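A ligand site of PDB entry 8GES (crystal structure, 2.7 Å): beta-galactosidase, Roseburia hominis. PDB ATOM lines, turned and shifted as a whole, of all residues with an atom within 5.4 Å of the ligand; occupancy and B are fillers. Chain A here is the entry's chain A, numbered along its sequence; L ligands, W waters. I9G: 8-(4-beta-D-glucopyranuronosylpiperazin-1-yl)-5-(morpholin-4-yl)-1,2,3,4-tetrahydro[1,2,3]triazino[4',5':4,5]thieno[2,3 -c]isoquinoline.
O04 of the ligand is in hydrogen-bond range of ND2 of Asn 378 (2.8 Å). NE2 of His 318 is in hydrogen-bond range of O01 of the ligand (2.8 Å). An oxygen (O04) of the ligand is in hydrogen-bond range of the side-chain carboxylate (OE2) of Glu 467 (2.8 Å). The indole nitrogen (NE1) of Trp 513 lies within hydrogen-bond range of an oxygen (O09) of the ligand. An oxygen (O09) of the ligand lies within hydrogen-bond range of the side-chain carboxylate of Asp 134, at 2.8 Å. NZ of Lys 534 is in salt-bridge range of O12 of the ligand (2.6 Å). ND2 of Asn 532 lies within hydrogen-bond range of O12 of the ligand. OH of Tyr 440 sits at hydrogen-bond distance from O11 of the ligand. The side-chain hydroxyl of Tyr 436 is in hydrogen-bond range of an oxygen (O06) of the ligand. An oxygen (O11) of the ligand is in salt-bridge range of the guanidinium group of Arg 523, at 3.0 Å. The side-chain carboxylate (OE2) of Glu 379 lies within salt-bridge range of a nitrogen (N13) of the ligand.
Merely in contact with the ligand: Met 382 (3.6 Å), Asn 434 (3.8 Å) and Phe 518 (3.5 Å). The nearest printed residue that does not touch the ligand is Gly 441 (4.2 Å).
Water W1 lies within hydrogen-bond range of N of Asp 134 and O01 of the ligand.
ND2 of Asn 434 lies within hydrogen-bond range of OE2 of Glu 379, at 3.4 Å. OH of Tyr 440 lies within hydrogen-bond range of NH2 of Arg 523 (3.2 Å). OD1 of Asn 378 sits close to OE2 of Glu 467. The side-chain carboxylate (OE1) of Glu 467 sits at hydrogen-bond distance from the side-chain hydroxyl (OH) of Tyr 436, at 2.7 Å. OD2 of Asp 134 lies within salt-bridge range of NH2 of Arg 523 (2.6 Å). NZ of Lys 534 lies within hydrogen-bond range of OH of Tyr 440 (2.9 Å). OE2 of Glu 467 lies within hydrogen-bond range of ND2 of Asn 434, 3.2 Å away. OD1 of Asn 378 sits at hydrogen-bond distance from ND2 of Asn 434 (2.9 Å).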
ATOM      1  N   ASP A 134     -22.778  32.586  -8.659  1.00  0.00           N
ATOM      2  CA  ASP A 134     -21.619  31.970  -8.002  1.00  0.00           C
ATOM      3  C   ASP A 134     -20.586  33.036  -7.635  1.00  0.00           C
ATOM      4  O   ASP A 134     -19.443  33.034  -8.096  1.00  0.00           O
ATOM      5  CB  ASP A 134     -21.025  30.892  -8.885  1.00  0.00           C
ATOM      6  CG  ASP A 134     -19.804  30.241  -8.270  1.00  0.00           C
ATOM      7  OD1 ASP A 134     -19.804  30.004  -7.048  1.00  0.00           O
ATOM      8  OD2 ASP A 134     -18.833  29.974  -9.022  1.00  0.00           O
ATOM      9  N   PHE A 135     -21.028  33.975  -6.805  1.00  0.00           N
ATOM     10  CA  PHE A 135     -20.139  34.986  -6.231  1.00  0.00           C
ATOM     11  C   PHE A 135     -20.874  35.706  -5.114  1.00  0.00           C
ATOM     12  O   PHE A 135     -22.106  35.780  -5.114  1.00  0.00           O
ATOM     13  CB  PHE A 135     -19.641  35.981  -7.295  1.00  0.00           C
ATOM     14  CG  PHE A 135     -20.714  36.869  -7.870  1.00  0.00           C
ATOM     15  CD1 PHE A 135     -21.016  38.071  -7.266  1.00  0.00           C
ATOM     16  CD2 PHE A 135     -21.380  36.517  -9.027  1.00  0.00           C
ATOM     17  CE1 PHE A 135     -21.994  38.904  -7.788  1.00  0.00           C
ATOM     18  CE2 PHE A 135     -22.355  37.348  -9.558  1.00  0.00           C
ATOM     19  CZ  PHE A 135     -22.665  38.539  -8.944  1.00  0.00           C
ATOM     20  N   HIS A 318     -19.578  39.990 -13.105  1.00  0.00           N
ATOM     21  CA  HIS A 318     -20.861  39.788 -13.794  1.00  0.00           C
ATOM     22  C   HIS A 318     -21.730  41.032 -13.670  1.00  0.00           C
ATOM     23  O   HIS A 318     -22.937  40.931 -13.454  1.00  0.00           O
ATOM     24  CB  HIS A 318     -21.638  38.605 -13.185  1.00  0.00           C
ATOM     25  CG  HIS A 318     -21.190  37.255 -13.655  1.00  0.00           C
ATOM     26  ND1 HIS A 318     -21.096  36.923 -14.989  1.00  0.00           N
ATOM     27  CD2 HIS A 318     -20.844  36.151 -12.954  1.00  0.00           C
ATOM     28  CE1 HIS A 318     -20.696  35.663 -15.090  1.00  0.00           C
ATOM     29  NE2 HIS A 318     -20.535  35.173 -13.868  1.00  0.00           N
ATOM     30  N   ILE A 343     -28.535  37.116 -14.179  1.00  0.00           N
ATOM     31  CA  ILE A 343     -27.838  35.811 -14.299  1.00  0.00           C
ATOM     32  C   ILE A 343     -28.582  34.627 -13.693  1.00  0.00           C
ATOM     33  O   ILE A 343     -29.418  34.847 -12.818  1.00  0.00           O
ATOM     34  CB  ILE A 343     -26.470  35.945 -13.599  1.00  0.00           C
ATOM     35  CG1 ILE A 343     -25.690  34.627 -13.615  1.00  0.00           C
ATOM     36  CG2 ILE A 343     -26.644  36.478 -12.185  1.00  0.00           C
ATOM     37  CD1 ILE A 343     -24.400  34.672 -12.832  1.00  0.00           C
ATOM     38  N   ASN A 378     -26.119  36.167 -18.209  1.00  0.00           N
ATOM     39  CA  ASN A 378     -25.175  35.053 -18.080  1.00  0.00           C
ATOM     40  C   ASN A 378     -25.937  33.830 -17.606  1.00  0.00           C
ATOM     41  O   ASN A 378     -26.480  33.823 -16.487  1.00  0.00           O
ATOM     42  CB  ASN A 378     -24.035  35.390 -17.115  1.00  0.00           C
ATOM     43  CG  ASN A 378     -23.188  34.173 -16.769  1.00  0.00           C
ATOM     44  OD1 ASN A 378     -22.249  33.828 -17.493  1.00  0.00           O
ATOM     45  ND2 ASN A 378     -23.510  33.522 -15.657  1.00  0.00           N
ATOM     46  N   GLU A 379     -25.995  32.794 -18.446  1.00  0.00           N
ATOM     47  CA  GLU A 379     -26.625  31.523 -18.101  1.00  0.00           C
ATOM     48  C   GLU A 379     -28.039  31.728 -17.582  1.00  0.00           C
ATOM     49  O   GLU A 379     -28.447  31.156 -16.567  1.00  0.00           O
ATOM     50  CB  GLU A 379     -25.782  30.756 -17.080  1.00  0.00           C
ATOM     51  CG  GLU A 379     -24.311  30.644 -17.425  1.00  0.00           C
ATOM     52  CD  GLU A 379     -23.532  29.796 -16.435  1.00  0.00           C
ATOM     53  OE1 GLU A 379     -23.955  29.723 -15.256  1.00  0.00           O
ATOM     54  OE2 GLU A 379     -22.520  29.203 -16.826  1.00  0.00           O
ATOM     55  N   MET A 382     -30.296  28.610 -17.237  1.00  0.00           N
ATOM     56  CA  MET A 382     -29.882  27.513 -16.376  1.00  0.00           C
ATOM     57  C   MET A 382     -31.093  26.780 -15.814  1.00  0.00           C
ATOM     58  O   MET A 382     -31.281  25.583 -16.039  1.00  0.00           O
ATOM     59  CB  MET A 382     -28.984  28.044 -15.252  1.00  0.00           C
ATOM     60  CG  MET A 382     -28.062  27.008 -14.621  1.00  0.00           C
ATOM     61  SD  MET A 382     -27.035  27.700 -13.311  1.00  0.00           S
ATOM     62  CE  MET A 382     -26.371  26.207 -12.569  1.00  0.00           C
ATOM     63  N   VAL A 415     -25.406  29.352 -20.890  1.00  0.00           N
ATOM     64  CA  VAL A 415     -25.013  28.172 -20.122  1.00  0.00           C
ATOM     65  C   VAL A 415     -24.723  27.024 -21.093  1.00  0.00           C
ATOM     66  O   VAL A 415     -25.210  26.988 -22.227  1.00  0.00           O
ATOM     67  CB  VAL A 415     -26.096  27.788 -19.096  1.00  0.00           C
ATOM     68  CG1 VAL A 415     -27.436  27.535 -19.789  1.00  0.00           C
ATOM     69  CG2 VAL A 415     -25.667  26.576 -18.283  1.00  0.00           C
ATOM     70  N   ASN A 434     -20.546  29.147 -22.236  1.00  0.00           N
ATOM     71  CA  ASN A 434     -19.731  28.860 -21.062  1.00  0.00           C
ATOM     72  C   ASN A 434     -19.599  27.348 -20.957  1.00  0.00           C
ATOM     73  O   ASN A 434     -20.551  26.660 -20.564  1.00  0.00           O
ATOM     74  CB  ASN A 434     -20.358  29.445 -19.801  1.00  0.00           C
ATOM     75  CG  ASN A 434     -20.486  30.951 -19.851  1.00  0.00           C
ATOM     76  OD1 ASN A 434     -19.943  31.605 -20.747  1.00  0.00           O
ATOM     77  ND2 ASN A 434     -21.218  31.522 -18.904  1.00  0.00           N
ATOM     78  N   TYR A 436     -17.381  23.852 -19.690  1.00  0.00           N
ATOM     79  CA  TYR A 436     -16.473  23.312 -18.696  1.00  0.00           C
ATOM     80  C   TYR A 436     -16.220  21.839 -18.958  1.00  0.00           C
ATOM     81  O   TYR A 436     -16.140  21.010 -18.045  1.00  0.00           O
ATOM     82  CB  TYR A 436     -17.026  23.547 -17.291  1.00  0.00           C
ATOM     83  CG  TYR A 436     -16.973  25.010 -16.918  1.00  0.00           C
ATOM     84  CD1 TYR A 436     -18.019  25.878 -17.222  1.00  0.00           C
ATOM     85  CD2 TYR A 436     -15.846  25.547 -16.295  1.00  0.00           C
ATOM     86  CE1 TYR A 436     -17.961  27.224 -16.897  1.00  0.00           C
ATOM     87  CE2 TYR A 436     -15.773  26.877 -15.964  1.00  0.00           C
ATOM     88  CZ  TYR A 436     -16.829  27.710 -16.265  1.00  0.00           C
ATOM     89  OH  TYR A 436     -16.737  29.047 -15.931  1.00  0.00           O
ATOM     90  N   TYR A 440     -16.414  20.018 -15.202  1.00  0.00           N
ATOM     91  CA  TYR A 440     -17.727  19.530 -14.781  1.00  0.00           C
ATOM     92  C   TYR A 440     -18.132  18.317 -15.615  1.00  0.00           C
ATOM     93  O   TYR A 440     -19.147  18.308 -16.321  1.00  0.00           O
ATOM     94  CB  TYR A 440     -18.769  20.634 -14.879  1.00  0.00           C
ATOM     95  CG  TYR A 440     -18.621  21.769 -13.880  1.00  0.00           C
ATOM     96  CD1 TYR A 440     -18.292  21.518 -12.550  1.00  0.00           C
ATOM     97  CD2 TYR A 440     -18.831  23.080 -14.266  1.00  0.00           C
ATOM     98  CE1 TYR A 440     -18.159  22.551 -11.640  1.00  0.00           C
ATOM     99  CE2 TYR A 440     -18.699  24.120 -13.368  1.00  0.00           C
ATOM    100  CZ  TYR A 440     -18.363  23.856 -12.055  1.00  0.00           C
ATOM    101  OH  TYR A 440     -18.240  24.893 -11.159  1.00  0.00           O
ATOM    102  N   GLY A 441     -17.310  17.272 -15.536  1.00  0.00           N
ATOM    103  CA  GLY A 441     -17.506  16.102 -16.362  1.00  0.00           C
ATOM    104  C   GLY A 441     -17.020  16.325 -17.785  1.00  0.00           C
ATOM    105  O   GLY A 441     -16.559  17.410 -18.154  1.00  0.00           O
ATOM    106  N   GLU A 467     -16.614  31.675 -21.198  1.00  0.00           N
ATOM    107  CA  GLU A 467     -16.199  31.102 -19.924  1.00  0.00           C
ATOM    108  C   GLU A 467     -15.675  29.696 -20.158  1.00  0.00           C
ATOM    109  O   GLU A 467     -16.389  28.843 -20.691  1.00  0.00           O
ATOM    110  CB  GLU A 467     -17.358  31.077 -18.920  1.00  0.00           C
ATOM    111  CG  GLU A 467     -17.495  32.337 -18.071  1.00  0.00           C
ATOM    112  CD  GLU A 467     -18.475  32.156 -16.914  1.00  0.00           C
ATOM    113  OE1 GLU A 467     -18.345  31.161 -16.167  1.00  0.00           O
ATOM    114  OE2 GLU A 467     -19.378  33.012 -16.757  1.00  0.00           O
ATOM    115  N   GLU A 471     -10.515  24.248 -11.673  1.00  0.00           N
ATOM    116  CA  GLU A 471     -10.071  24.602 -10.337  1.00  0.00           C
ATOM    117  C   GLU A 471      -8.616  24.209 -10.123  1.00  0.00           C
ATOM    118  O   GLU A 471      -8.108  23.251 -10.726  1.00  0.00           O
ATOM    119  CB  GLU A 471     -10.949  23.944  -9.276  1.00  0.00           C
ATOM    120  CG  GLU A 471     -12.436  24.153  -9.504  1.00  0.00           C
ATOM    121  CD  GLU A 471     -12.972  25.379  -8.823  1.00  0.00           C
ATOM    122  OE1 GLU A 471     -12.239  25.984  -8.020  1.00  0.00           O
ATOM    123  OE2 GLU A 471     -14.145  25.748  -9.083  1.00  0.00           O
ATOM    124  N   TRP A 513     -11.941  31.765 -17.401  1.00  0.00           N
ATOM    125  CA  TRP A 513     -12.595  31.910 -16.106  1.00  0.00           C
ATOM    126  C   TRP A 513     -11.746  31.180 -15.070  1.00  0.00           C
ATOM    127  O   TRP A 513     -11.553  29.966 -15.174  1.00  0.00           O
ATOM    128  CB  TRP A 513     -14.009  31.341 -16.141  1.00  0.00           C
ATOM    129  CG  TRP A 513     -14.808  31.662 -14.912  1.00  0.00           C
ATOM    130  CD1 TRP A 513     -15.023  30.863 -13.832  1.00  0.00           C
ATOM    131  CD2 TRP A 513     -15.510  32.883 -14.652  1.00  0.00           C
ATOM    132  NE1 TRP A 513     -15.800  31.513 -12.899  1.00  0.00           N
ATOM    133  CE2 TRP A 513     -16.121  32.756 -13.380  1.00  0.00           C
ATOM    134  CE3 TRP A 513     -15.675  34.084 -15.352  1.00  0.00           C
ATOM    135  CZ2 TRP A 513     -16.877  33.770 -12.813  1.00  0.00           C
ATOM    136  CZ3 TRP A 513     -16.438  35.086 -14.783  1.00  0.00           C
ATOM    137  CH2 TRP A 513     -17.027  34.930 -13.522  1.00  0.00           C
ATOM    138  N   PHE A 518     -11.793  34.087  -6.486  1.00  0.00           N
ATOM    139  CA  PHE A 518     -12.727  35.137  -6.080  1.00  0.00           C
ATOM    140  C   PHE A 518     -13.667  34.625  -5.008  1.00  0.00           C
ATOM    141  O   PHE A 518     -13.732  33.421  -4.724  1.00  0.00           O
ATOM    142  CB  PHE A 518     -13.520  35.658  -7.283  1.00  0.00           C
ATOM    143  CG  PHE A 518     -14.280  34.599  -8.027  1.00  0.00           C
ATOM    144  CD1 PHE A 518     -15.584  34.270  -7.666  1.00  0.00           C
ATOM    145  CD2 PHE A 518     -13.708  33.959  -9.102  1.00  0.00           C
ATOM    146  CE1 PHE A 518     -16.287  33.304  -8.362  1.00  0.00           C
ATOM    147  CE2 PHE A 518     -14.399  32.995  -9.807  1.00  0.00           C
ATOM    148  CZ  PHE A 518     -15.693  32.669  -9.444  1.00  0.00           C
ATOM    149  N   ARG A 523     -19.435  28.131  -1.915  1.00  0.00           N
ATOM    150  CA  ARG A 523     -18.546  27.051  -2.305  1.00  0.00           C
ATOM    151  C   ARG A 523     -17.924  26.390  -1.072  1.00  0.00           C
ATOM    152  O   ARG A 523     -17.644  27.039  -0.068  1.00  0.00           O
ATOM    153  CB  ARG A 523     -17.444  27.577  -3.218  1.00  0.00           C
ATOM    154  CG  ARG A 523     -17.950  28.147  -4.522  1.00  0.00           C
ATOM    155  CD  ARG A 523     -18.093  27.047  -5.558  1.00  0.00           C
ATOM    156  NE  ARG A 523     -18.487  27.543  -6.864  1.00  0.00           N
ATOM    157  CZ  ARG A 523     -18.398  26.842  -7.995  1.00  0.00           C
ATOM    158  NH1 ARG A 523     -17.921  25.608  -7.959  1.00  0.00           N
ATOM    159  NH2 ARG A 523     -18.789  27.379  -9.142  1.00  0.00           N
ATOM    160  N   ASN A 532     -14.074  30.422  -5.179  1.00  0.00           N
ATOM    161  CA  ASN A 532     -13.874  29.742  -6.444  1.00  0.00           C
ATOM    162  C   ASN A 532     -12.396  29.789  -6.766  1.00  0.00           C
ATOM    163  O   ASN A 532     -11.784  30.859  -6.776  1.00  0.00           O
ATOM    164  CB  ASN A 532     -14.696  30.397  -7.554  1.00  0.00           C
ATOM    165  CG  ASN A 532     -14.577  29.668  -8.871  1.00  0.00           C
ATOM    166  OD1 ASN A 532     -13.494  29.553  -9.449  1.00  0.00           O
ATOM    167  ND2 ASN A 532     -15.702  29.155  -9.362  1.00  0.00           N
ATOM    168  N   LYS A 534     -10.773  28.787  -9.610  1.00  0.00           N
ATOM    169  CA  LYS A 534     -10.531  28.595 -11.030  1.00  0.00           C
ATOM    170  C   LYS A 534      -9.596  29.647 -11.621  1.00  0.00           C
ATOM    171  O   LYS A 534      -9.370  29.653 -12.832  1.00  0.00           O
ATOM    172  CB  LYS A 534     -11.867  28.608 -11.782  1.00  0.00           C
ATOM    173  CG  LYS A 534     -12.756  27.406 -11.497  1.00  0.00           C
ATOM    174  CD  LYS A 534     -13.924  27.341 -12.457  1.00  0.00           C
ATOM    175  CE  LYS A 534     -14.832  26.158 -12.159  1.00  0.00           C
ATOM    176  NZ  LYS A 534     -15.756  26.458 -11.037  1.00  0.00           N
HETATM  177  C02 I9G L   1     -19.881  31.735 -13.161  1.00  0.00           C
HETATM  178  C03 I9G L   1     -20.900  31.065 -13.974  1.00  0.00           C
HETATM  179  C05 I9G L   1     -20.532  29.668 -14.578  1.00  0.00           C
HETATM  180  C07 I9G L   1     -18.415  29.723 -13.122  1.00  0.00           C
HETATM  181  C08 I9G L   1     -19.226  30.722 -12.251  1.00  0.00           C
HETATM  182  C10 I9G L   1     -17.895  28.626 -12.258  1.00  0.00           C
HETATM  183  C14 I9G L   1     -21.212  27.535 -14.823  1.00  0.00           C
HETATM  184  C15 I9G L   1     -22.296  26.479 -14.494  1.00  0.00           C
HETATM  185  C17 I9G L   1     -22.915  27.802 -12.578  1.00  0.00           C
HETATM  186  C18 I9G L   1     -21.688  28.668 -12.933  1.00  0.00           C
HETATM  187  C19 I9G L   1     -22.372  25.368 -12.230  1.00  0.00           C
HETATM  188  C23 I9G L   1     -21.935  22.999 -11.752  1.00  0.00           C
HETATM  189  C24 I9G L   1     -22.447  23.968 -12.663  1.00  0.00           C
HETATM  190  C26 I9G L   1     -22.636  21.502 -13.526  1.00  0.00           C
HETATM  191  C27 I9G L   1     -22.048  21.590 -12.264  1.00  0.00           C
HETATM  192  C28 I9G L   1     -21.623  20.379 -11.567  1.00  0.00           C
HETATM  193  C29 I9G L   1     -21.816  19.166 -12.186  1.00  0.00           C
HETATM  194  C30 I9G L   1     -21.385  17.829 -11.526  1.00  0.00           C
HETATM  195  C31 I9G L   1     -20.465  17.989 -10.286  1.00  0.00           C
HETATM  196  C32 I9G L   1     -20.865  19.189  -9.402  1.00  0.00           C
HETATM  197  C33 I9G L   1     -20.991  20.494 -10.164  1.00  0.00           C
HETATM  198  C34 I9G L   1     -22.426  19.166 -13.500  1.00  0.00           C
HETATM  199  C37 I9G L   1     -21.493  17.318 -14.935  1.00  0.00           C
HETATM  200  C38 I9G L   1     -21.715  15.876 -15.362  1.00  0.00           C
HETATM  201  C40 I9G L   1     -24.023  16.226 -15.426  1.00  0.00           C
HETATM  202  C41 I9G L   1     -23.848  17.677 -14.991  1.00  0.00           C
HETATM  203  N13 I9G L   1     -21.462  28.770 -14.276  1.00  0.00           N
HETATM  204  N16 I9G L   1     -22.853  26.465 -13.138  1.00  0.00           N
HETATM  205  N20 I9G L   1     -21.838  25.655 -11.049  1.00  0.00           N
HETATM  206  N21 I9G L   1     -21.378  24.691 -10.223  1.00  0.00           N
HETATM  207  N22 I9G L   1     -21.425  23.411 -10.557  1.00  0.00           N
HETATM  208  N35 I9G L   1     -22.794  20.296 -14.118  1.00  0.00           N
HETATM  209  N36 I9G L   1     -22.629  17.896 -14.205  1.00  0.00           N
HETATM  210  O01 I9G L   1     -20.564  32.764 -12.414  1.00  0.00           O
HETATM  211  O04 I9G L   1     -21.328  31.855 -15.094  1.00  0.00           O
HETATM  212  O06 I9G L   1     -19.161  29.105 -14.216  1.00  0.00           O
HETATM  213  O09 I9G L   1     -18.372  31.427 -11.409  1.00  0.00           O
HETATM  214  O11 I9G L   1     -18.559  27.560 -12.125  1.00  0.00           O
HETATM  215  O12 I9G L   1     -16.790  28.740 -11.666  1.00  0.00           O
HETATM  216  O39 I9G L   1     -22.898  15.700 -16.064  1.00  0.00           O
HETATM  217  S25 I9G L   1     -23.008  23.129 -14.039  1.00  0.00           S
HETATM  218  O   HOH W   1     -23.084  31.843 -11.351  1.00  0.00           O
